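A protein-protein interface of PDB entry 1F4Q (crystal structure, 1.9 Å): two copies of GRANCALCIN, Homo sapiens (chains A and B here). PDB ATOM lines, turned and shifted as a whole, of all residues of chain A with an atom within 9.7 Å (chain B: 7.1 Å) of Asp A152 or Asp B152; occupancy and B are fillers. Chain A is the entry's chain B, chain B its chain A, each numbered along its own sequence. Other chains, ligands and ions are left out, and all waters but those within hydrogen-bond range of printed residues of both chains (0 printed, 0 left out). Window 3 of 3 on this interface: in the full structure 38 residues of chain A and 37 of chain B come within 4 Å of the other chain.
The backbone NH (N) of Tyr A155 is in hydrogen-bond range of the backbone carbonyl oxygen (O) of Gly B149 (2.9 Å).
The side-chain hydroxyl (OG) of Ser B150 is in hydrogen-bond range of the side-chain carboxylate (OD1) of Asp A152, at 2.7 Å.
OG of Ser B150 lies close to O of Phe A153 (3.2 Å).
The backbone NH (N) of Ala B151 lies close to the side-chain carboxylate (OD1) of Asp A152 (3.4 Å).
The backbone carbonyl oxygen (O) of Ala B151 sits at hydrogen-bond distance from the backbone NH (N) of Phe A153, 2.8 Å away.
O of Ala A151 lies within hydrogen-bond range of N of Phe B153, at 2.8 Å.
The side-chain carboxylate of Asp B152 lies close to the side-chain carboxylate of Asp A152 (3.1 Å).
The backbone NH (N) of Gly B149 sits at hydrogen-bond distance from the side-chain carboxylate (OD2) of Asp B144.
The backbone NH (N) of Gly A149 lies within hydrogen-bond range of the side-chain carboxylate (OD2) of Asp A144.
Among the printed residues, merely in contact across the chains: Phe A140 with Phe B153, Gly A149 with Ile B154, Ser A150 with Phe B153, Ala A151 with Ala B151, Ala A151 with Asp B152, Phe A153 with Phe B140, Phe A153 with Phe B153, Ile A154 with Gly B149, Tyr A155 with Phe B140, Phe A158 with Phe B140 and Phe A158 with Phe B153.
Printed residues of chain B within 4 Å of Phe A140: Phe B153 (3.7 Å).
Of chain B, only Ser B150 (2.7 Å), Ala B151 (3.3 Å) and Asp B152 (3.1 Å) come within 4 Å of Asp A152.
Printed residues of chain B within 4 Å of Ile A154: Gly B149 (3.7 Å).
Of the printed residues of chain B, Phe A158 touches Phe B140 (3.4 Å) and Phe B153 (3.99 Å).
Printed residues of chain A within 4 Å of Ala B151: Ala A151, Asp A152 and Phe A153.
Of chain A, only Ala A151 (3.3 Å) and Asp A152 (3.1 Å) come within 4 Å of Asp B152.
The nearest residue of chain A that does not touch Asp B152 is Phe A153 (4.8 Å).
Of the 11 printed residues of chain B, 7 touch a printed residue of chain A.
Hydrophobic or aromatic side chains of chain B that line the printed part of chain A: Phe B140, Phe B153 and Ile B154.
Of the 19 printed residues of chain A, 9 touch a printed residue of chain B.
Printed residues of chain A that touch a printed residue of chain B: Phe A140, Gly A149, Ser A150, Ala A151, Asp A152, Phe A153, Ile A154, Tyr A155 and Phe A158.
Hydrophobic or aromatic side chains of chain A within 4 Å of the printed part of chain B: Phe A140, Phe A153, Tyr A155 and Phe A158.
Among the printed residues, 18 pairs touch across the chains.
Among the printed residues, no Asp or Glu carboxylate lies within 4 Å of a Lys or Arg side-chain nitrogen of the other chain.
Ala A151 touches Asp B152, and with the chains exchanged Asp A152 touches Ala B151.
Asp A152 touches Ser B150, but with the chains exchanged Ser A150 does not touch Asp B152 (6.2 Å).
Asp B152 touches its own counterpart, Asp A152.
Phe B153 touches its own counterpart, Phe A153.
11 positions are printed for both chains.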
ATOM      1  N   PHE A 139      -3.367   3.113 -29.315  1.00  0.00           N
ATOM      2  CA  PHE A 139      -2.376   2.050 -29.367  1.00  0.00           C
ATOM      3  C   PHE A 139      -1.158   2.426 -28.513  1.00  0.00           C
ATOM      4  O   PHE A 139      -0.684   1.629 -27.702  1.00  0.00           O
ATOM      5  CB  PHE A 139      -1.959   1.830 -30.828  1.00  0.00           C
ATOM      6  CG  PHE A 139      -0.818   0.872 -31.014  1.00  0.00           C
ATOM      7  CD1 PHE A 139      -0.985  -0.493 -30.796  1.00  0.00           C
ATOM      8  CD2 PHE A 139       0.424   1.336 -31.446  1.00  0.00           C
ATOM      9  CE1 PHE A 139       0.069  -1.386 -31.010  1.00  0.00           C
ATOM     10  CE2 PHE A 139       1.485   0.454 -31.663  1.00  0.00           C
ATOM     11  CZ  PHE A 139       1.307  -0.912 -31.446  1.00  0.00           C
ATOM     12  N   PHE A 140      -0.665   3.646 -28.696  1.00  0.00           N
ATOM     13  CA  PHE A 140       0.501   4.117 -27.954  1.00  0.00           C
ATOM     14  C   PHE A 140       0.249   4.149 -26.445  1.00  0.00           C
ATOM     15  O   PHE A 140       1.025   3.594 -25.667  1.00  0.00           O
ATOM     16  CB  PHE A 140       0.909   5.512 -28.445  1.00  0.00           C
ATOM     17  CG  PHE A 140       2.137   6.064 -27.764  1.00  0.00           C
ATOM     18  CD1 PHE A 140       2.037   6.743 -26.550  1.00  0.00           C
ATOM     19  CD2 PHE A 140       3.395   5.895 -28.335  1.00  0.00           C
ATOM     20  CE1 PHE A 140       3.177   7.247 -25.913  1.00  0.00           C
ATOM     21  CE2 PHE A 140       4.545   6.397 -27.706  1.00  0.00           C
ATOM     22  CZ  PHE A 140       4.431   7.072 -26.493  1.00  0.00           C
ATOM     23  N   LYS A 141      -0.842   4.793 -26.045  1.00  0.00           N
ATOM     24  CA  LYS A 141      -1.208   4.917 -24.640  1.00  0.00           C
ATOM     25  C   LYS A 141      -1.197   3.599 -23.868  1.00  0.00           C
ATOM     26  O   LYS A 141      -0.855   3.577 -22.684  1.00  0.00           O
ATOM     27  CB  LYS A 141      -2.589   5.564 -24.518  1.00  0.00           C
ATOM     28  CG  LYS A 141      -3.072   5.741 -23.085  1.00  0.00           C
ATOM     29  CD  LYS A 141      -4.434   6.413 -23.051  1.00  0.00           C
ATOM     30  CE  LYS A 141      -4.380   7.783 -23.709  1.00  0.00           C
ATOM     31  NZ  LYS A 141      -5.723   8.408 -23.806  1.00  0.00           N
ATOM     32  N   LYS A 142      -1.573   2.509 -24.533  1.00  0.00           N
ATOM     33  CA  LYS A 142      -1.603   1.196 -23.893  1.00  0.00           C
ATOM     34  C   LYS A 142      -0.212   0.666 -23.553  1.00  0.00           C
ATOM     35  O   LYS A 142      -0.065  -0.181 -22.670  1.00  0.00           O
ATOM     36  CB  LYS A 142      -2.331   0.182 -24.786  1.00  0.00           C
ATOM     37  CG  LYS A 142      -3.839   0.354 -24.822  1.00  0.00           C
ATOM     38  CD  LYS A 142      -4.494  -0.672 -25.746  1.00  0.00           C
ATOM     39  CE  LYS A 142      -6.012  -0.634 -25.637  1.00  0.00           C
ATOM     40  NZ  LYS A 142      -6.579   0.694 -26.000  1.00  0.00           N
ATOM     41  N   ARG A 143       0.805   1.158 -24.257  1.00  0.00           N
ATOM     42  CA  ARG A 143       2.176   0.727 -24.010  1.00  0.00           C
ATOM     43  C   ARG A 143       2.934   1.703 -23.116  1.00  0.00           C
ATOM     44  O   ARG A 143       4.051   1.416 -22.686  1.00  0.00           O
ATOM     45  CB  ARG A 143       2.934   0.551 -25.330  1.00  0.00           C
ATOM     46  CG  ARG A 143       2.653  -0.758 -26.052  1.00  0.00           C
ATOM     47  CD  ARG A 143       1.238  -0.801 -26.579  1.00  0.00           C
ATOM     48  NE  ARG A 143       0.962  -2.026 -27.325  1.00  0.00           N
ATOM     49  CZ  ARG A 143      -0.216  -2.303 -27.876  1.00  0.00           C
ATOM     50  NH1 ARG A 143      -1.215  -1.439 -27.761  1.00  0.00           N
ATOM     51  NH2 ARG A 143      -0.396  -3.443 -28.531  1.00  0.00           N
ATOM     52  N   ASP A 144       2.321   2.857 -22.857  1.00  0.00           N
ATOM     53  CA  ASP A 144       2.897   3.893 -22.001  1.00  0.00           C
ATOM     54  C   ASP A 144       2.395   3.585 -20.590  1.00  0.00           C
ATOM     55  O   ASP A 144       1.535   4.286 -20.060  1.00  0.00           O
ATOM     56  CB  ASP A 144       2.392   5.273 -22.436  1.00  0.00           C
ATOM     57  CG  ASP A 144       3.014   6.403 -21.644  1.00  0.00           C
ATOM     58  OD1 ASP A 144       3.731   6.116 -20.667  1.00  0.00           O
ATOM     59  OD2 ASP A 144       2.784   7.581 -21.996  1.00  0.00           O
ATOM     60  N   HIS A 145       2.939   2.531 -19.998  1.00  0.00           N
ATOM     61  CA  HIS A 145       2.537   2.080 -18.667  1.00  0.00           C
ATOM     62  C   HIS A 145       2.729   3.088 -17.535  1.00  0.00           C
ATOM     63  O   HIS A 145       1.904   3.158 -16.625  1.00  0.00           O
ATOM     64  CB  HIS A 145       3.268   0.779 -18.329  1.00  0.00           C
ATOM     65  CG  HIS A 145       3.088  -0.297 -19.355  1.00  0.00           C
ATOM     66  ND1 HIS A 145       1.846  -0.744 -19.756  1.00  0.00           N
ATOM     67  CD2 HIS A 145       3.992  -1.014 -20.064  1.00  0.00           C
ATOM     68  CE1 HIS A 145       1.994  -1.689 -20.668  1.00  0.00           C
ATOM     69  NE2 HIS A 145       3.286  -1.872 -20.874  1.00  0.00           N
ATOM     70  N   LEU A 146       3.808   3.866 -17.579  1.00  0.00           N
ATOM     71  CA  LEU A 146       4.053   4.845 -16.523  1.00  0.00           C
ATOM     72  C   LEU A 146       3.395   6.189 -16.786  1.00  0.00           C
ATOM     73  O   LEU A 146       3.549   7.116 -15.990  1.00  0.00           O
ATOM     74  CB  LEU A 146       5.560   5.066 -16.311  1.00  0.00           C
ATOM     75  CG  LEU A 146       6.438   3.988 -15.660  1.00  0.00           C
ATOM     76  CD1 LEU A 146       5.585   3.048 -14.809  1.00  0.00           C
ATOM     77  CD2 LEU A 146       7.179   3.214 -16.740  1.00  0.00           C
ATOM     78  N   GLN A 148       4.004   8.558 -19.173  1.00  0.00           N
ATOM     79  CA  GLN A 148       5.071   9.555 -19.291  1.00  0.00           C
ATOM     80  C   GLN A 148       5.153  10.255 -20.652  1.00  0.00           C
ATOM     81  O   GLN A 148       5.841  11.267 -20.791  1.00  0.00           O
ATOM     82  CB  GLN A 148       6.426   8.890 -19.027  1.00  0.00           C
ATOM     83  CG  GLN A 148       6.599   8.255 -17.648  1.00  0.00           C
ATOM     84  CD  GLN A 148       6.571   9.277 -16.526  1.00  0.00           C
ATOM     85  OE1 GLN A 148       7.260  10.296 -16.585  1.00  0.00           O
ATOM     86  NE2 GLN A 148       5.781   9.006 -15.493  1.00  0.00           N
ATOM     87  N   GLY A 149       4.467   9.718 -21.654  1.00  0.00           N
ATOM     88  CA  GLY A 149       4.544  10.313 -22.977  1.00  0.00           C
ATOM     89  C   GLY A 149       5.603   9.565 -23.763  1.00  0.00           C
ATOM     90  O   GLY A 149       6.099  10.039 -24.791  1.00  0.00           O
ATOM     91  N   SER A 150       5.961   8.388 -23.252  1.00  0.00           N
ATOM     92  CA  SER A 150       6.948   7.520 -23.888  1.00  0.00           C
ATOM     93  C   SER A 150       6.524   6.062 -23.735  1.00  0.00           C
ATOM     94  O   SER A 150       5.758   5.715 -22.833  1.00  0.00           O
ATOM     95  CB  SER A 150       8.332   7.706 -23.254  1.00  0.00           C
ATOM     96  OG  SER A 150       8.335   7.299 -21.894  1.00  0.00           O
ATOM     97  N   ALA A 151       7.035   5.210 -24.614  1.00  0.00           N
ATOM     98  CA  ALA A 151       6.716   3.788 -24.574  1.00  0.00           C
ATOM     99  C   ALA A 151       7.819   2.978 -25.232  1.00  0.00           C
ATOM    100  O   ALA A 151       8.449   3.430 -26.188  1.00  0.00           O
ATOM    101  CB  ALA A 151       5.380   3.521 -25.282  1.00  0.00           C
ATOM    102  N   ASP A 152       8.048   1.776 -24.709  1.00  0.00           N
ATOM    103  CA  ASP A 152       9.068   0.880 -25.235  1.00  0.00           C
ATOM    104  C   ASP A 152       8.341  -0.286 -25.913  1.00  0.00           C
ATOM    105  O   ASP A 152       7.625  -1.041 -25.261  1.00  0.00           O
ATOM    106  CB  ASP A 152       9.952   0.391 -24.081  1.00  0.00           C
ATOM    107  CG  ASP A 152      11.089  -0.498 -24.543  1.00  0.00           C
ATOM    108  OD1 ASP A 152      11.545  -0.345 -25.693  1.00  0.00           O
ATOM    109  OD2 ASP A 152      11.543  -1.341 -23.739  1.00  0.00           O
ATOM    110  N   PHE A 153       8.519  -0.420 -27.224  1.00  0.00           N
ATOM    111  CA  PHE A 153       7.844  -1.477 -27.977  1.00  0.00           C
ATOM    112  C   PHE A 153       8.716  -2.641 -28.406  1.00  0.00           C
ATOM    113  O   PHE A 153       9.870  -2.463 -28.797  1.00  0.00           O
ATOM    114  CB  PHE A 153       7.221  -0.924 -29.267  1.00  0.00           C
ATOM    115  CG  PHE A 153       6.171   0.120 -29.058  1.00  0.00           C
ATOM    116  CD1 PHE A 153       6.526   1.444 -28.834  1.00  0.00           C
ATOM    117  CD2 PHE A 153       4.822  -0.210 -29.145  1.00  0.00           C
ATOM    118  CE1 PHE A 153       5.555   2.425 -28.707  1.00  0.00           C
ATOM    119  CE2 PHE A 153       3.842   0.765 -29.019  1.00  0.00           C
ATOM    120  CZ  PHE A 153       4.208   2.087 -28.800  1.00  0.00           C
ATOM    121  N   ILE A 154       8.150  -3.842 -28.343  1.00  0.00           N
ATOM    122  CA  ILE A 154       8.843  -5.026 -28.822  1.00  0.00           C
ATOM    123  C   ILE A 154       8.460  -5.025 -30.310  1.00  0.00           C
ATOM    124  O   ILE A 154       7.296  -4.798 -30.649  1.00  0.00           O
ATOM    125  CB  ILE A 154       8.310  -6.305 -28.143  1.00  0.00           C
ATOM    126  CG1 ILE A 154       8.572  -6.235 -26.633  1.00  0.00           C
ATOM    127  CG2 ILE A 154       8.985  -7.525 -28.739  1.00  0.00           C
ATOM    128  CD1 ILE A 154       7.988  -7.397 -25.844  1.00  0.00           C
ATOM    129  N   TYR A 155       9.428  -5.265 -31.188  1.00  0.00           N
ATOM    130  CA  TYR A 155       9.188  -5.240 -32.632  1.00  0.00           C
ATOM    131  C   TYR A 155       7.896  -5.872 -33.154  1.00  0.00           C
ATOM    132  O   TYR A 155       7.157  -5.231 -33.905  1.00  0.00           O
ATOM    133  CB  TYR A 155      10.375  -5.850 -33.372  1.00  0.00           C
ATOM    134  CG  TYR A 155      10.208  -5.889 -34.878  1.00  0.00           C
ATOM    135  CD1 TYR A 155       9.944  -7.089 -35.536  1.00  0.00           C
ATOM    136  CD2 TYR A 155      10.344  -4.734 -35.648  1.00  0.00           C
ATOM    137  CE1 TYR A 155       9.827  -7.143 -36.930  1.00  0.00           C
ATOM    138  CE2 TYR A 155      10.227  -4.775 -37.045  1.00  0.00           C
ATOM    139  CZ  TYR A 155       9.973  -5.986 -37.677  1.00  0.00           C
ATOM    140  OH  TYR A 155       9.898  -6.057 -39.056  1.00  0.00           O
ATOM    141  N   ASP A 156       7.626  -7.119 -32.780  1.00  0.00           N
ATOM    142  CA  ASP A 156       6.420  -7.797 -33.255  1.00  0.00           C
ATOM    143  C   ASP A 156       5.126  -7.107 -32.806  1.00  0.00           C
ATOM    144  O   ASP A 156       4.132  -7.109 -33.538  1.00  0.00           O
ATOM    145  CB  ASP A 156       6.425  -9.264 -32.801  1.00  0.00           C
ATOM    146  CG  ASP A 156       5.317 -10.083 -33.449  1.00  0.00           C
ATOM    147  OD1 ASP A 156       4.217 -10.176 -32.866  1.00  0.00           O
ATOM    148  OD2 ASP A 156       5.545 -10.623 -34.553  1.00  0.00           O
ATOM    149  N   ASP A 157       5.138  -6.519 -31.612  1.00  0.00           N
ATOM    150  CA  ASP A 157       3.962  -5.821 -31.086  1.00  0.00           C
ATOM    151  C   ASP A 157       3.803  -4.496 -31.828  1.00  0.00           C
ATOM    152  O   ASP A 157       2.688  -4.072 -32.157  1.00  0.00           O
ATOM    153  CB  ASP A 157       4.122  -5.562 -29.582  1.00  0.00           C
ATOM    154  CG  ASP A 157       2.912  -4.875 -28.972  1.00  0.00           C
ATOM    155  OD1 ASP A 157       1.776  -5.333 -29.221  1.00  0.00           O
ATOM    156  OD2 ASP A 157       3.093  -3.885 -28.227  1.00  0.00           O
ATOM    157  N   PHE A 158       4.931  -3.845 -32.078  1.00  0.00           N
ATOM    158  CA  PHE A 158       4.934  -2.584 -32.805  1.00  0.00           C
ATOM    159  C   PHE A 158       4.392  -2.792 -34.221  1.00  0.00           C
ATOM    160  O   PHE A 158       3.498  -2.064 -34.662  1.00  0.00           O
ATOM    161  CB  PHE A 158       6.352  -2.031 -32.885  1.00  0.00           C
ATOM    162  CG  PHE A 158       6.477  -0.830 -33.771  1.00  0.00           C
ATOM    163  CD1 PHE A 158       6.154   0.436 -33.298  1.00  0.00           C
ATOM    164  CD2 PHE A 158       6.896  -0.967 -35.090  1.00  0.00           C
ATOM    165  CE1 PHE A 158       6.249   1.546 -34.120  1.00  0.00           C
ATOM    166  CE2 PHE A 158       6.993   0.149 -35.923  1.00  0.00           C
ATOM    167  CZ  PHE A 158       6.669   1.398 -35.437  1.00  0.00           C
ATOM    168  N   PHE B 140      11.394   1.715 -37.182  1.00  0.00           N
ATOM    169  CA  PHE B 140      11.605   1.065 -35.893  1.00  0.00           C
ATOM    170  C   PHE B 140      13.084   0.784 -35.637  1.00  0.00           C
ATOM    171  O   PHE B 140      13.606   1.077 -34.562  1.00  0.00           O
ATOM    172  CB  PHE B 140      10.813  -0.244 -35.841  1.00  0.00           C
ATOM    173  CG  PHE B 140      10.933  -0.978 -34.534  1.00  0.00           C
ATOM    174  CD1 PHE B 140      12.038  -1.783 -34.266  1.00  0.00           C
ATOM    175  CD2 PHE B 140       9.932  -0.875 -33.574  1.00  0.00           C
ATOM    176  CE1 PHE B 140      12.139  -2.478 -33.058  1.00  0.00           C
ATOM    177  CE2 PHE B 140      10.024  -1.567 -32.364  1.00  0.00           C
ATOM    178  CZ  PHE B 140      11.131  -2.370 -32.109  1.00  0.00           C
ATOM    179  N   ARG B 143      15.296   3.438 -34.022  1.00  0.00           N
ATOM    180  CA  ARG B 143      15.159   3.756 -32.599  1.00  0.00           C
ATOM    181  C   ARG B 143      15.713   2.631 -31.724  1.00  0.00           C
ATOM    182  O   ARG B 143      15.885   2.800 -30.514  1.00  0.00           O
ATOM    183  CB  ARG B 143      13.691   4.009 -32.226  1.00  0.00           C
ATOM    184  CG  ARG B 143      13.167   5.414 -32.548  1.00  0.00           C
ATOM    185  CD  ARG B 143      13.085   5.667 -34.049  1.00  0.00           C
ATOM    186  NE  ARG B 143      12.625   7.022 -34.363  1.00  0.00           N
ATOM    187  CZ  ARG B 143      12.595   7.533 -35.590  1.00  0.00           C
ATOM    188  NH1 ARG B 143      12.997   6.800 -36.621  1.00  0.00           N
ATOM    189  NH2 ARG B 143      12.177   8.778 -35.790  1.00  0.00           N
ATOM    190  N   ASP B 144      15.979   1.485 -32.338  1.00  0.00           N
ATOM    191  CA  ASP B 144      16.519   0.333 -31.626  1.00  0.00           C
ATOM    192  C   ASP B 144      18.043   0.408 -31.657  1.00  0.00           C
ATOM    193  O   ASP B 144      18.705  -0.333 -32.381  1.00  0.00           O
ATOM    194  CB  ASP B 144      16.026  -0.958 -32.285  1.00  0.00           C
ATOM    195  CG  ASP B 144      16.587  -2.209 -31.631  1.00  0.00           C
ATOM    196  OD1 ASP B 144      16.906  -2.177 -30.423  1.00  0.00           O
ATOM    197  OD2 ASP B 144      16.691  -3.235 -32.331  1.00  0.00           O
ATOM    198  N   HIS B 145      18.593   1.314 -30.857  1.00  0.00           N
ATOM    199  CA  HIS B 145      20.035   1.514 -30.806  1.00  0.00           C
ATOM    200  C   HIS B 145      20.835   0.327 -30.283  1.00  0.00           C
ATOM    201  O   HIS B 145      21.903   0.031 -30.807  1.00  0.00           O
ATOM    202  CB  HIS B 145      20.353   2.765 -29.983  1.00  0.00           C
ATOM    203  CG  HIS B 145      19.714   4.008 -30.520  1.00  0.00           C
ATOM    204  ND1 HIS B 145      19.879   4.424 -31.824  1.00  0.00           N
ATOM    205  CD2 HIS B 145      18.893   4.913 -29.937  1.00  0.00           C
ATOM    206  CE1 HIS B 145      19.185   5.531 -32.021  1.00  0.00           C
ATOM    207  NE2 HIS B 145      18.577   5.849 -30.892  1.00  0.00           N
ATOM    208  N   GLY B 149      15.750  -5.526 -30.434  1.00  0.00           N
ATOM    209  CA  GLY B 149      14.476  -5.929 -31.004  1.00  0.00           C
ATOM    210  C   GLY B 149      13.362  -5.204 -30.273  1.00  0.00           C
ATOM    211  O   GLY B 149      12.187  -5.572 -30.348  1.00  0.00           O
ATOM    212  N   SER B 150      13.753  -4.167 -29.540  1.00  0.00           N
ATOM    213  CA  SER B 150      12.826  -3.338 -28.776  1.00  0.00           C
ATOM    214  C   SER B 150      13.220  -1.887 -29.043  1.00  0.00           C
ATOM    215  O   SER B 150      14.374  -1.609 -29.358  1.00  0.00           O
ATOM    216  CB  SER B 150      12.940  -3.651 -27.280  1.00  0.00           C
ATOM    217  OG  SER B 150      12.094  -2.814 -26.508  1.00  0.00           O
ATOM    218  N   ALA B 151      12.269  -0.966 -28.919  1.00  0.00           N
ATOM    219  CA  ALA B 151      12.563   0.438 -29.174  1.00  0.00           C
ATOM    220  C   ALA B 151      11.663   1.407 -28.431  1.00  0.00           C
ATOM    221  O   ALA B 151      10.442   1.223 -28.363  1.00  0.00           O
ATOM    222  CB  ALA B 151      12.482   0.718 -30.672  1.00  0.00           C
ATOM    223  N   ASP B 152      12.283   2.448 -27.879  1.00  0.00           N
ATOM    224  CA  ASP B 152      11.578   3.502 -27.155  1.00  0.00           C
ATOM    225  C   ASP B 152      11.071   4.523 -28.165  1.00  0.00           C
ATOM    226  O   ASP B 152      11.731   4.787 -29.170  1.00  0.00           O
ATOM    227  CB  ASP B 152      12.527   4.269 -26.224  1.00  0.00           C
ATOM    228  CG  ASP B 152      12.980   3.464 -25.027  1.00  0.00           C
ATOM    229  OD1 ASP B 152      14.012   3.858 -24.433  1.00  0.00           O
ATOM    230  OD2 ASP B 152      12.316   2.473 -24.667  1.00  0.00           O
ATOM    231  N   PHE B 153       9.912   5.103 -27.881  1.00  0.00           N
ATOM    232  CA  PHE B 153       9.359   6.155 -28.716  1.00  0.00           C
ATOM    233  C   PHE B 153       8.762   7.215 -27.817  1.00  0.00           C
ATOM    234  O   PHE B 153       8.060   6.902 -26.860  1.00  0.00           O
ATOM    235  CB  PHE B 153       8.250   5.642 -29.641  1.00  0.00           C
ATOM    236  CG  PHE B 153       8.742   4.792 -30.769  1.00  0.00           C
ATOM    237  CD1 PHE B 153       8.799   3.407 -30.640  1.00  0.00           C
ATOM    238  CD2 PHE B 153       9.151   5.374 -31.967  1.00  0.00           C
ATOM    239  CE1 PHE B 153       9.257   2.613 -31.692  1.00  0.00           C
ATOM    240  CE2 PHE B 153       9.608   4.595 -33.019  1.00  0.00           C
ATOM    241  CZ  PHE B 153       9.662   3.209 -32.885  1.00  0.00           C
ATOM    242  N   ILE B 154       9.077   8.472 -28.095  1.00  0.00           N
ATOM    243  CA  ILE B 154       8.475   9.556 -27.346  1.00  0.00           C
ATOM    244  C   ILE B 154       7.225   9.776 -28.207  1.00  0.00           C
ATOM    245  O   ILE B 154       7.315   9.729 -29.432  1.00  0.00           O
ATOM    246  CB  ILE B 154       9.374  10.800 -27.346  1.00  0.00           C
ATOM    247  CG1 ILE B 154      10.659  10.500 -26.558  1.00  0.00           C
ATOM    248  CG2 ILE B 154       8.617  11.977 -26.762  1.00  0.00           C
ATOM    249  CD1 ILE B 154      11.712  11.583 -26.659  1.00  0.00           C
ATOM    250  N   ASP B 157       7.327  11.717 -31.569  1.00  0.00           N
ATOM    251  CA  ASP B 157       8.169  11.080 -32.591  1.00  0.00           C
ATOM    252  C   ASP B 157       7.442   9.877 -33.194  1.00  0.00           C
ATOM    253  O   ASP B 157       7.500   9.626 -34.406  1.00  0.00           O
ATOM    254  CB  ASP B 157       9.505  10.632 -31.975  1.00  0.00           C
ATOM    255  CG  ASP B 157      10.403   9.919 -32.975  1.00  0.00           C
ATOM    256  OD1 ASP B 157      10.574  10.433 -34.098  1.00  0.00           O
ATOM    257  OD2 ASP B 157      10.950   8.848 -32.641  1.00  0.00           O
